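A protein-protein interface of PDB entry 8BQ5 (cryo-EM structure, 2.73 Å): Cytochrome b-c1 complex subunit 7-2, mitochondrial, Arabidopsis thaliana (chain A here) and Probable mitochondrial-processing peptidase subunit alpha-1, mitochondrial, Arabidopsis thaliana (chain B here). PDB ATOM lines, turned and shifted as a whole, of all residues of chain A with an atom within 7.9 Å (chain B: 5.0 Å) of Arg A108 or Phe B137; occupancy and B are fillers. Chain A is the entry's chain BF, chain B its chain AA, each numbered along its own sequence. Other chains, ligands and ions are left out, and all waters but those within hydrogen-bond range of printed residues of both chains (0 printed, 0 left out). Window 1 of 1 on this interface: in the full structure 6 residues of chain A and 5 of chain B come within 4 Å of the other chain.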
ATOM      1  N   VAL A 101      -3.068 -16.707 -12.423  1.00  0.00           N
ATOM      2  CA  VAL A 101      -1.900 -16.519 -11.570  1.00  0.00           C
ATOM      3  C   VAL A 101      -1.345 -17.867 -11.123  1.00  0.00           C
ATOM      4  O   VAL A 101      -0.127 -18.073 -11.084  1.00  0.00           O
ATOM      5  CB  VAL A 101      -2.258 -15.619 -10.372  1.00  0.00           C
ATOM      6  CG1 VAL A 101      -1.265 -15.804  -9.238  1.00  0.00           C
ATOM      7  CG2 VAL A 101      -2.313 -14.164 -10.803  1.00  0.00           C
ATOM      8  N   LYS A 102      -2.232 -18.806 -10.786  1.00  0.00           N
ATOM      9  CA  LYS A 102      -1.794 -20.149 -10.420  1.00  0.00           C
ATOM     10  C   LYS A 102      -1.138 -20.861 -11.597  1.00  0.00           C
ATOM     11  O   LYS A 102      -0.163 -21.599 -11.418  1.00  0.00           O
ATOM     12  CB  LYS A 102      -2.978 -20.960  -9.894  1.00  0.00           C
ATOM     13  CG  LYS A 102      -3.568 -20.427  -8.602  1.00  0.00           C
ATOM     14  CD  LYS A 102      -4.256 -21.523  -7.806  1.00  0.00           C
ATOM     15  CE  LYS A 102      -5.759 -21.515  -8.040  1.00  0.00           C
ATOM     16  NZ  LYS A 102      -6.114 -21.801  -9.458  1.00  0.00           N
ATOM     17  N   ARG A 103      -1.673 -20.669 -12.806  1.00  0.00           N
ATOM     18  CA  ARG A 103      -1.071 -21.279 -13.987  1.00  0.00           C
ATOM     19  C   ARG A 103       0.335 -20.746 -14.228  1.00  0.00           C
ATOM     20  O   ARG A 103       1.249 -21.509 -14.558  1.00  0.00           O
ATOM     21  CB  ARG A 103      -1.951 -21.034 -15.214  1.00  0.00           C
ATOM     22  CG  ARG A 103      -2.471 -22.300 -15.874  1.00  0.00           C
ATOM     23  CD  ARG A 103      -3.924 -22.148 -16.296  1.00  0.00           C
ATOM     24  NE  ARG A 103      -4.175 -20.864 -16.942  1.00  0.00           N
ATOM     25  CZ  ARG A 103      -5.262 -20.129 -16.750  1.00  0.00           C
ATOM     26  NH1 ARG A 103      -6.223 -20.518 -15.929  1.00  0.00           N
ATOM     27  NH2 ARG A 103      -5.388 -18.975 -17.398  1.00  0.00           N
ATOM     28  N   GLU A 104       0.524 -19.432 -14.077  1.00  0.00           N
ATOM     29  CA  GLU A 104       1.850 -18.848 -14.248  1.00  0.00           C
ATOM     30  C   GLU A 104       2.813 -19.335 -13.175  1.00  0.00           C
ATOM     31  O   GLU A 104       3.994 -19.573 -13.452  1.00  0.00           O
ATOM     32  CB  GLU A 104       1.754 -17.322 -14.234  1.00  0.00           C
ATOM     33  CG  GLU A 104       1.788 -16.693 -15.613  1.00  0.00           C
ATOM     34  CD  GLU A 104       0.804 -15.552 -15.756  1.00  0.00           C
ATOM     35  OE1 GLU A 104       0.634 -14.787 -14.784  1.00  0.00           O
ATOM     36  OE2 GLU A 104       0.201 -15.420 -16.841  1.00  0.00           O
ATOM     37  N   ARG A 105       2.328 -19.479 -11.939  1.00  0.00           N
ATOM     38  CA  ARG A 105       3.176 -19.961 -10.853  1.00  0.00           C
ATOM     39  C   ARG A 105       3.661 -21.378 -11.123  1.00  0.00           C
ATOM     40  O   ARG A 105       4.833 -21.701 -10.899  1.00  0.00           O
ATOM     41  CB  ARG A 105       2.410 -19.906  -9.533  1.00  0.00           C
ATOM     42  CG  ARG A 105       2.304 -18.526  -8.926  1.00  0.00           C
ATOM     43  CD  ARG A 105       3.339 -18.331  -7.838  1.00  0.00           C
ATOM     44  NE  ARG A 105       2.744 -18.395  -6.509  1.00  0.00           N
ATOM     45  CZ  ARG A 105       3.383 -18.809  -5.423  1.00  0.00           C
ATOM     46  NH1 ARG A 105       4.651 -19.188  -5.469  1.00  0.00           N
ATOM     47  NH2 ARG A 105       2.736 -18.843  -4.262  1.00  0.00           N
ATOM     48  N   ALA A 106       2.764 -22.246 -11.596  1.00  0.00           N
ATOM     49  CA  ALA A 106       3.143 -23.628 -11.869  1.00  0.00           C
ATOM     50  C   ALA A 106       4.127 -23.711 -13.027  1.00  0.00           C
ATOM     51  O   ALA A 106       5.045 -24.540 -13.014  1.00  0.00           O
ATOM     52  CB  ALA A 106       1.898 -24.466 -12.155  1.00  0.00           C
ATOM     53  N   GLU A 107       3.948 -22.862 -14.041  1.00  0.00           N
ATOM     54  CA  GLU A 107       4.860 -22.860 -15.180  1.00  0.00           C
ATOM     55  C   GLU A 107       6.264 -22.441 -14.760  1.00  0.00           C
ATOM     56  O   GLU A 107       7.257 -22.998 -15.241  1.00  0.00           O
ATOM     57  CB  GLU A 107       4.316 -21.941 -16.274  1.00  0.00           C
ATOM     58  CG  GLU A 107       5.261 -21.699 -17.437  1.00  0.00           C
ATOM     59  CD  GLU A 107       4.775 -20.595 -18.356  1.00  0.00           C
ATOM     60  OE1 GLU A 107       4.650 -19.443 -17.890  1.00  0.00           O
ATOM     61  OE2 GLU A 107       4.513 -20.880 -19.543  1.00  0.00           O
ATOM     62  N   ARG A 108       6.366 -21.457 -13.861  1.00  0.00           N
ATOM     63  CA  ARG A 108       7.668 -21.070 -13.325  1.00  0.00           C
ATOM     64  C   ARG A 108       8.313 -22.222 -12.566  1.00  0.00           C
ATOM     65  O   ARG A 108       9.513 -22.481 -12.714  1.00  0.00           O
ATOM     66  CB  ARG A 108       7.515 -19.857 -12.410  1.00  0.00           C
ATOM     67  CG  ARG A 108       7.462 -18.522 -13.121  1.00  0.00           C
ATOM     68  CD  ARG A 108       7.541 -17.381 -12.120  1.00  0.00           C
ATOM     69  NE  ARG A 108       8.916 -17.011 -11.810  1.00  0.00           N
ATOM     70  CZ  ARG A 108       9.670 -16.232 -12.572  1.00  0.00           C
ATOM     71  NH1 ARG A 108       9.212 -15.720 -13.702  1.00  0.00           N
ATOM     72  NH2 ARG A 108      10.914 -15.958 -12.191  1.00  0.00           N
ATOM     73  N   GLU A 109       7.529 -22.921 -11.742  1.00  0.00           N
ATOM     74  CA  GLU A 109       8.062 -24.033 -10.963  1.00  0.00           C
ATOM     75  C   GLU A 109       8.515 -25.177 -11.862  1.00  0.00           C
ATOM     76  O   GLU A 109       9.539 -25.817 -11.594  1.00  0.00           O
ATOM     77  CB  GLU A 109       7.010 -24.509  -9.960  1.00  0.00           C
ATOM     78  CG  GLU A 109       7.186 -25.939  -9.478  1.00  0.00           C
ATOM     79  CD  GLU A 109       5.865 -26.612  -9.159  1.00  0.00           C
ATOM     80  OE1 GLU A 109       4.988 -26.657 -10.049  1.00  0.00           O
ATOM     81  OE2 GLU A 109       5.702 -27.095  -8.020  1.00  0.00           O
ATOM     82  N   ALA A 110       7.769 -25.447 -12.936  1.00  0.00           N
ATOM     83  CA  ALA A 110       8.113 -26.551 -13.826  1.00  0.00           C
ATOM     84  C   ALA A 110       9.442 -26.323 -14.534  1.00  0.00           C
ATOM     85  O   ALA A 110      10.171 -27.284 -14.803  1.00  0.00           O
ATOM     86  CB  ALA A 110       7.002 -26.765 -14.853  1.00  0.00           C
ATOM     87  N   LEU A 111       9.770 -25.074 -14.853  1.00  0.00           N
ATOM     88  CA  LEU A 111      11.000 -24.755 -15.564  1.00  0.00           C
ATOM     89  C   LEU A 111      12.152 -24.403 -14.630  1.00  0.00           C
ATOM     90  O   LEU A 111      13.231 -24.042 -15.108  1.00  0.00           O
ATOM     91  CB  LEU A 111      10.755 -23.614 -16.552  1.00  0.00           C
ATOM     92  CG  LEU A 111      10.039 -24.028 -17.838  1.00  0.00           C
ATOM     93  CD1 LEU A 111       9.791 -22.825 -18.729  1.00  0.00           C
ATOM     94  CD2 LEU A 111      10.845 -25.083 -18.575  1.00  0.00           C
ATOM     95  N   GLY A 112      11.951 -24.501 -13.318  1.00  0.00           N
ATOM     96  CA  GLY A 112      13.030 -24.281 -12.377  1.00  0.00           C
ATOM     97  C   GLY A 112      13.351 -22.838 -12.071  1.00  0.00           C
ATOM     98  O   GLY A 112      14.492 -22.535 -11.713  1.00  0.00           O
ATOM     99  N   ALA A 113      12.386 -21.936 -12.197  1.00  0.00           N
ATOM    100  CA  ALA A 113      12.610 -20.531 -11.899  1.00  0.00           C
ATOM    101  C   ALA A 113      12.235 -20.217 -10.454  1.00  0.00           C
ATOM    102  O   ALA A 113      11.456 -20.928  -9.817  1.00  0.00           O
ATOM    103  CB  ALA A 113      11.810 -19.641 -12.848  1.00  0.00           C
ATOM    104  N   LEU A 114      12.813 -19.134  -9.943  1.00  0.00           N
ATOM    105  CA  LEU A 114      12.482 -18.670  -8.607  1.00  0.00           C
ATOM    106  C   LEU A 114      11.064 -18.100  -8.581  1.00  0.00           C
ATOM    107  O   LEU A 114      10.586 -17.558  -9.580  1.00  0.00           O
ATOM    108  CB  LEU A 114      13.472 -17.602  -8.151  1.00  0.00           C
ATOM    109  CG  LEU A 114      14.910 -18.056  -7.910  1.00  0.00           C
ATOM    110  CD1 LEU A 114      15.794 -16.862  -7.601  1.00  0.00           C
ATOM    111  CD2 LEU A 114      14.961 -19.069  -6.780  1.00  0.00           C
ATOM    112  N   PRO A 115      10.369 -18.216  -7.450  1.00  0.00           N
ATOM    113  CA  PRO A 115       9.026 -17.635  -7.355  1.00  0.00           C
ATOM    114  C   PRO A 115       9.077 -16.119  -7.456  1.00  0.00           C
ATOM    115  O   PRO A 115      10.047 -15.479  -7.047  1.00  0.00           O
ATOM    116  CB  PRO A 115       8.535 -18.084  -5.972  1.00  0.00           C
ATOM    117  CG  PRO A 115       9.467 -19.169  -5.544  1.00  0.00           C
ATOM    118  CD  PRO A 115      10.772 -18.888  -6.204  1.00  0.00           C
ATOM    119  N   LEU A 116       8.014 -15.545  -8.015  1.00  0.00           N
ATOM    120  CA  LEU A 116       7.909 -14.095  -8.086  1.00  0.00           C
ATOM    121  C   LEU A 116       7.575 -13.464  -6.743  1.00  0.00           C
ATOM    122  O   LEU A 116       7.689 -12.241  -6.606  1.00  0.00           O
ATOM    123  CB  LEU A 116       6.857 -13.689  -9.119  1.00  0.00           C
ATOM    124  CG  LEU A 116       7.234 -13.861 -10.591  1.00  0.00           C
ATOM    125  CD1 LEU A 116       6.105 -13.378 -11.481  1.00  0.00           C
ATOM    126  CD2 LEU A 116       8.525 -13.128 -10.911  1.00  0.00           C
ATOM    127  N   TYR A 117       7.168 -14.260  -5.758  1.00  0.00           N
ATOM    128  CA  TYR A 117       6.801 -13.764  -4.439  1.00  0.00           C
ATOM    129  C   TYR A 117       6.729 -14.949  -3.489  1.00  0.00           C
ATOM    130  O   TYR A 117       6.358 -16.059  -3.881  1.00  0.00           O
ATOM    131  CB  TYR A 117       5.465 -13.014  -4.471  1.00  0.00           C
ATOM    132  CG  TYR A 117       4.426 -13.685  -5.336  1.00  0.00           C
ATOM    133  CD1 TYR A 117       3.658 -14.729  -4.848  1.00  0.00           C
ATOM    134  CD2 TYR A 117       4.227 -13.282  -6.649  1.00  0.00           C
ATOM    135  CE1 TYR A 117       2.713 -15.346  -5.635  1.00  0.00           C
ATOM    136  CE2 TYR A 117       3.287 -13.898  -7.446  1.00  0.00           C
ATOM    137  CZ  TYR A 117       2.532 -14.928  -6.935  1.00  0.00           C
ATOM    138  OH  TYR A 117       1.592 -15.542  -7.725  1.00  0.00           O
ATOM    139  N   THR B 135       3.642 -16.858 -22.571  1.00  0.00           N
ATOM    140  CA  THR B 135       3.841 -15.825 -21.567  1.00  0.00           C
ATOM    141  C   THR B 135       5.211 -15.176 -21.726  1.00  0.00           C
ATOM    142  O   THR B 135       6.067 -15.651 -22.476  1.00  0.00           O
ATOM    143  CB  THR B 135       3.708 -16.408 -20.161  1.00  0.00           C
ATOM    144  OG1 THR B 135       4.787 -17.318 -19.915  1.00  0.00           O
ATOM    145  CG2 THR B 135       2.388 -17.143 -20.012  1.00  0.00           C
ATOM    146  N   HIS B 136       5.407 -14.069 -21.006  1.00  0.00           N
ATOM    147  CA  HIS B 136       6.710 -13.414 -20.987  1.00  0.00           C
ATOM    148  C   HIS B 136       7.786 -14.360 -20.471  1.00  0.00           C
ATOM    149  O   HIS B 136       8.888 -14.432 -21.029  1.00  0.00           O
ATOM    150  CB  HIS B 136       6.650 -12.157 -20.120  1.00  0.00           C
ATOM    151  CG  HIS B 136       7.815 -11.237 -20.309  1.00  0.00           C
ATOM    152  ND1 HIS B 136       7.948 -10.053 -19.615  1.00  0.00           N
ATOM    153  CD2 HIS B 136       8.899 -11.323 -21.115  1.00  0.00           C
ATOM    154  CE1 HIS B 136       9.066  -9.454 -19.981  1.00  0.00           C
ATOM    155  NE2 HIS B 136       9.662 -10.204 -20.891  1.00  0.00           N
ATOM    156  N   PHE B 137       7.480 -15.097 -19.403  1.00  0.00           N
ATOM    157  CA  PHE B 137       8.459 -16.009 -18.819  1.00  0.00           C
ATOM    158  C   PHE B 137       8.863 -17.091 -19.811  1.00  0.00           C
ATOM    159  O   PHE B 137      10.051 -17.392 -19.972  1.00  0.00           O
ATOM    160  CB  PHE B 137       7.894 -16.629 -17.544  1.00  0.00           C
ATOM    161  CG  PHE B 137       8.690 -17.790 -17.033  1.00  0.00           C
ATOM    162  CD1 PHE B 137       9.945 -17.597 -16.484  1.00  0.00           C
ATOM    163  CD2 PHE B 137       8.188 -19.076 -17.106  1.00  0.00           C
ATOM    164  CE1 PHE B 137      10.680 -18.663 -16.016  1.00  0.00           C
ATOM    165  CE2 PHE B 137       8.920 -20.146 -16.639  1.00  0.00           C
ATOM    166  CZ  PHE B 137      10.168 -19.938 -16.093  1.00  0.00           C
ATOM    167  N   ARG B 138       7.882 -17.689 -20.490  1.00  0.00           N
ATOM    168  CA  ARG B 138       8.187 -18.716 -21.479  1.00  0.00           C
ATOM    169  C   ARG B 138       8.963 -18.138 -22.655  1.00  0.00           C
ATOM    170  O   ARG B 138       9.907 -18.761 -23.154  1.00  0.00           O
ATOM    171  CB  ARG B 138       6.897 -19.377 -21.959  1.00  0.00           C
ATOM    172  CG  ARG B 138       7.104 -20.404 -23.052  1.00  0.00           C
ATOM    173  CD  ARG B 138       5.782 -20.983 -23.515  1.00  0.00           C
ATOM    174  NE  ARG B 138       5.949 -21.841 -24.681  1.00  0.00           N
ATOM    175  CZ  ARG B 138       6.224 -23.136 -24.624  1.00  0.00           C
ATOM    176  NH1 ARG B 138       6.366 -23.761 -23.468  1.00  0.00           N
ATOM    177  NH2 ARG B 138       6.362 -23.820 -25.756  1.00  0.00           N
ATOM    178  N   LEU B 139       8.580 -16.944 -23.111  1.00  0.00           N
ATOM    179  CA  LEU B 139       9.235 -16.342 -24.267  1.00  0.00           C
ATOM    180  C   LEU B 139      10.695 -16.019 -23.975  1.00  0.00           C
ATOM    181  O   LEU B 139      11.561 -16.186 -24.841  1.00  0.00           O
ATOM    182  CB  LEU B 139       8.472 -15.090 -24.698  1.00  0.00           C
ATOM    183  CG  LEU B 139       9.010 -14.319 -25.899  1.00  0.00           C
ATOM    184  CD1 LEU B 139       8.906 -15.171 -27.138  1.00  0.00           C
ATOM    185  CD2 LEU B 139       8.221 -13.042 -26.079  1.00  0.00           C
ATOM    186  N   VAL B 140      10.988 -15.547 -22.761  1.00  0.00           N
ATOM    187  CA  VAL B 140      12.374 -15.281 -22.385  1.00  0.00           C
ATOM    188  C   VAL B 140      13.164 -16.582 -22.314  1.00  0.00           C
ATOM    189  O   VAL B 140      14.342 -16.633 -22.689  1.00  0.00           O
ATOM    190  CB  VAL B 140      12.425 -14.506 -21.052  1.00  0.00           C
ATOM    191  CG1 VAL B 140      13.847 -14.430 -20.525  1.00  0.00           C
ATOM    192  CG2 VAL B 140      11.857 -13.113 -21.231  1.00  0.00           C
ATOM    193  N   ARG B 141      12.526 -17.657 -21.846  1.00  0.00           N
ATOM    194  CA  ARG B 141      13.223 -18.932 -21.714  1.00  0.00           C
ATOM    195  C   ARG B 141      13.509 -19.565 -23.072  1.00  0.00           C
ATOM    196  O   ARG B 141      14.554 -20.202 -23.253  1.00  0.00           O
ATOM    197  CB  ARG B 141      12.412 -19.884 -20.836  1.00  0.00           C
ATOM    198  CG  ARG B 141      12.514 -19.588 -19.350  1.00  0.00           C
ATOM    199  CD  ARG B 141      13.944 -19.733 -18.857  1.00  0.00           C
ATOM    200  NE  ARG B 141      14.130 -19.149 -17.535  1.00  0.00           N
ATOM    201  CZ  ARG B 141      14.244 -19.850 -16.415  1.00  0.00           C
ATOM    202  NH1 ARG B 141      14.198 -21.171 -16.419  1.00  0.00           N
ATOM    203  NH2 ARG B 141      14.407 -19.208 -15.262  1.00  0.00           N
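The side-chain hydroxyl (OG1) of Thr B135 is in hydrogen-bond range of the side-chain carboxylate (OE1) of Glu A107 (2.9 Å). The guanidinium group of Arg B141 lies within hydrogen-bond range of the backbone carbonyl oxygen of Leu A111.
The backbone NH (N) of Arg B138 sits at hydrogen-bond distance from the side-chain hydroxyl (OG1) of Thr B135, at 3.2 Å. The backbone carbonyl oxygen of Arg A108 lies within hydrogen-bond range of the backbone NH of Ala A113 (3.0 Å). O of Leu A114 sits at hydrogen-bond distance from NE of Arg A108 (2.8 Å).
Among the printed residues, merely in contact across the chains: Arg A108 with Phe B137, Ala A113 with Phe B137, Leu A111 with Phe B137, Ala A113 with Arg B141, Glu A107 with Phe B137 and Glu A107 with Arg B138.
Arg A108 touches just one residue of chain B: Phe B137 (3.4 Å). Of chain A, only Glu A107 (3.6 Å), Arg A108 (3.4 Å), Leu A111 (3.5 Å) and Ala A113 (3.5 Å) come within 4 Å of Phe B137. Of the printed residues of chain B, Leu A111 touches Phe B137 and Arg B141. Of the printed residues of chain A, Arg B141 touches Leu A111 and Ala A113. Printed residues of chain B within 4 Å of Glu A107: Thr B135, Phe B137 and Arg B138. The nearest printed residue of chain A that does not touch Arg B138 is Leu A111 (5.2 Å).
Hydrophobic or aromatic side chains of chain B that line the printed part of chain A: Phe B137. Hydrophobic or aromatic side chains of chain A that line the printed part of chain B: Leu A111 and Ala A113. Among the printed residues, 8 pairs touch across the chains.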
